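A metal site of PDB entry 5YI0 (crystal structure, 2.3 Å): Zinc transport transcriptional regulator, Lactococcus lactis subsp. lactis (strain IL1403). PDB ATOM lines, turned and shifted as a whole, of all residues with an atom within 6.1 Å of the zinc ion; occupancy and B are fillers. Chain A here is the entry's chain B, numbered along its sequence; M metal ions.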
ATOM      1  N   HIS A  23      -9.604  -4.052 -19.064  1.00  0.00           N
ATOM      2  CA  HIS A  23     -10.871  -3.350 -18.860  1.00  0.00           C
ATOM      3  C   HIS A  23     -11.144  -2.357 -19.995  1.00  0.00           C
ATOM      4  O   HIS A  23     -12.277  -2.256 -20.487  1.00  0.00           O
ATOM      5  CB  HIS A  23     -10.886  -2.634 -17.506  1.00  0.00           C
ATOM      6  CG  HIS A  23     -12.162  -1.906 -17.218  1.00  0.00           C
ATOM      7  ND1 HIS A  23     -13.401  -2.490 -17.365  1.00  0.00           N
ATOM      8  CD2 HIS A  23     -12.392  -0.634 -16.799  1.00  0.00           C
ATOM      9  CE1 HIS A  23     -14.343  -1.610 -17.044  1.00  0.00           C
ATOM     10  NE2 HIS A  23     -13.753  -0.487 -16.697  1.00  0.00           N
ATOM     11  N   GLU A  24     -10.098  -1.636 -20.397  1.00  0.00           N
ATOM     12  CA  GLU A  24     -10.156  -0.735 -21.534  1.00  0.00           C
ATOM     13  C   GLU A  24      -8.906  -0.905 -22.389  1.00  0.00           C
ATOM     14  O   GLU A  24      -8.008  -1.669 -22.039  1.00  0.00           O
ATOM     15  CB  GLU A  24     -10.240   0.711 -21.060  1.00  0.00           C
ATOM     16  CG  GLU A  24     -11.321   0.987 -20.025  1.00  0.00           C
ATOM     17  CD  GLU A  24     -11.184   2.373 -19.420  1.00  0.00           C
ATOM     18  OE1 GLU A  24     -11.738   3.336 -20.013  1.00  0.00           O
ATOM     19  OE2 GLU A  24     -10.502   2.485 -18.368  1.00  0.00           O
ATOM     20  N   LEU A  26      -5.712   0.755 -23.183  1.00  0.00           N
ATOM     21  CA  LEU A  26      -4.808   1.798 -22.729  1.00  0.00           C
ATOM     22  C   LEU A  26      -3.359   1.386 -22.921  1.00  0.00           C
ATOM     23  O   LEU A  26      -3.034   0.211 -22.822  1.00  0.00           O
ATOM     24  CB  LEU A  26      -5.028   2.081 -21.245  1.00  0.00           C
ATOM     25  CG  LEU A  26      -6.341   2.747 -20.848  1.00  0.00           C
ATOM     26  CD1 LEU A  26      -6.474   2.634 -19.320  1.00  0.00           C
ATOM     27  CD2 LEU A  26      -6.382   4.202 -21.328  1.00  0.00           C
ATOM     28  N   GLU A  41     -17.293   5.871 -14.708  1.00  0.00           N
ATOM     29  CA  GLU A  41     -15.996   6.478 -14.944  1.00  0.00           C
ATOM     30  C   GLU A  41     -16.139   7.914 -15.435  1.00  0.00           C
ATOM     31  O   GLU A  41     -15.411   8.812 -14.983  1.00  0.00           O
ATOM     32  CB  GLU A  41     -15.187   5.632 -15.928  1.00  0.00           C
ATOM     33  CG  GLU A  41     -13.922   6.332 -16.380  1.00  0.00           C
ATOM     34  CD  GLU A  41     -12.890   5.395 -16.993  1.00  0.00           C
ATOM     35  OE1 GLU A  41     -12.020   5.910 -17.735  1.00  0.00           O
ATOM     36  OE2 GLU A  41     -12.945   4.175 -16.740  1.00  0.00           O
ATOM     37  N   MET A  45     -14.851  11.184 -13.418  1.00  0.00           N
ATOM     38  CA  MET A  45     -13.972  12.141 -14.056  1.00  0.00           C
ATOM     39  C   MET A  45     -14.609  13.506 -14.028  1.00  0.00           C
ATOM     40  O   MET A  45     -13.955  14.498 -13.737  1.00  0.00           O
ATOM     41  CB  MET A  45     -13.656  11.717 -15.501  1.00  0.00           C
ATOM     42  CG  MET A  45     -12.782  10.469 -15.609  1.00  0.00           C
ATOM     43  SD  MET A  45     -11.271  10.624 -14.631  1.00  0.00           S
ATOM     44  CE  MET A  45     -10.583   8.983 -14.730  1.00  0.00           C
ATOM     45  N   HIS A 108      -5.629   7.784 -13.202  1.00  0.00           N
ATOM     46  CA  HIS A 108      -6.290   7.075 -14.286  1.00  0.00           C
ATOM     47  C   HIS A 108      -6.575   7.976 -15.471  1.00  0.00           C
ATOM     48  O   HIS A 108      -6.551   7.531 -16.621  1.00  0.00           O
ATOM     49  CB  HIS A 108      -7.565   6.401 -13.804  1.00  0.00           C
ATOM     50  CG  HIS A 108      -8.246   5.576 -14.855  1.00  0.00           C
ATOM     51  ND1 HIS A 108      -8.028   4.223 -14.986  1.00  0.00           N
ATOM     52  CD2 HIS A 108      -9.124   5.918 -15.823  1.00  0.00           C
ATOM     53  CE1 HIS A 108      -8.749   3.761 -16.000  1.00  0.00           C
ATOM     54  NE2 HIS A 108      -9.429   4.768 -16.506  1.00  0.00           N
ATOM     55  N   HIS A 112      -5.186   7.755 -19.552  1.00  0.00           N
ATOM     56  CA  HIS A 112      -5.948   8.074 -20.764  1.00  0.00           C
ATOM     57  C   HIS A 112      -5.243   9.133 -21.576  1.00  0.00           C
ATOM     58  O   HIS A 112      -5.190   9.062 -22.802  1.00  0.00           O
ATOM     59  CB  HIS A 112      -7.364   8.556 -20.427  1.00  0.00           C
ATOM     60  CG  HIS A 112      -8.306   7.440 -20.120  1.00  0.00           C
ATOM     61  ND1 HIS A 112      -9.001   6.767 -21.108  1.00  0.00           N
ATOM     62  CD2 HIS A 112      -8.656   6.849 -18.951  1.00  0.00           C
ATOM     63  CE1 HIS A 112      -9.746   5.816 -20.552  1.00  0.00           C
ATOM     64  NE2 HIS A 112      -9.564   5.864 -19.241  1.00  0.00           N
HETATM   65 ZN    ZN M   1     -10.485   4.556 -18.157  1.00  0.00          ZN
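Of the 7 residues printed, 4 come within 4 Å of the zinc ion. The nearest printed residue that does not touch the zinc ion is Leu 26 (4.6 Å).
The zinc ion is bound by NE2 of His 112, NE2 of His 108, OE2 of Glu 24, OE1 of Glu 41 and OE1 of Glu 24.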
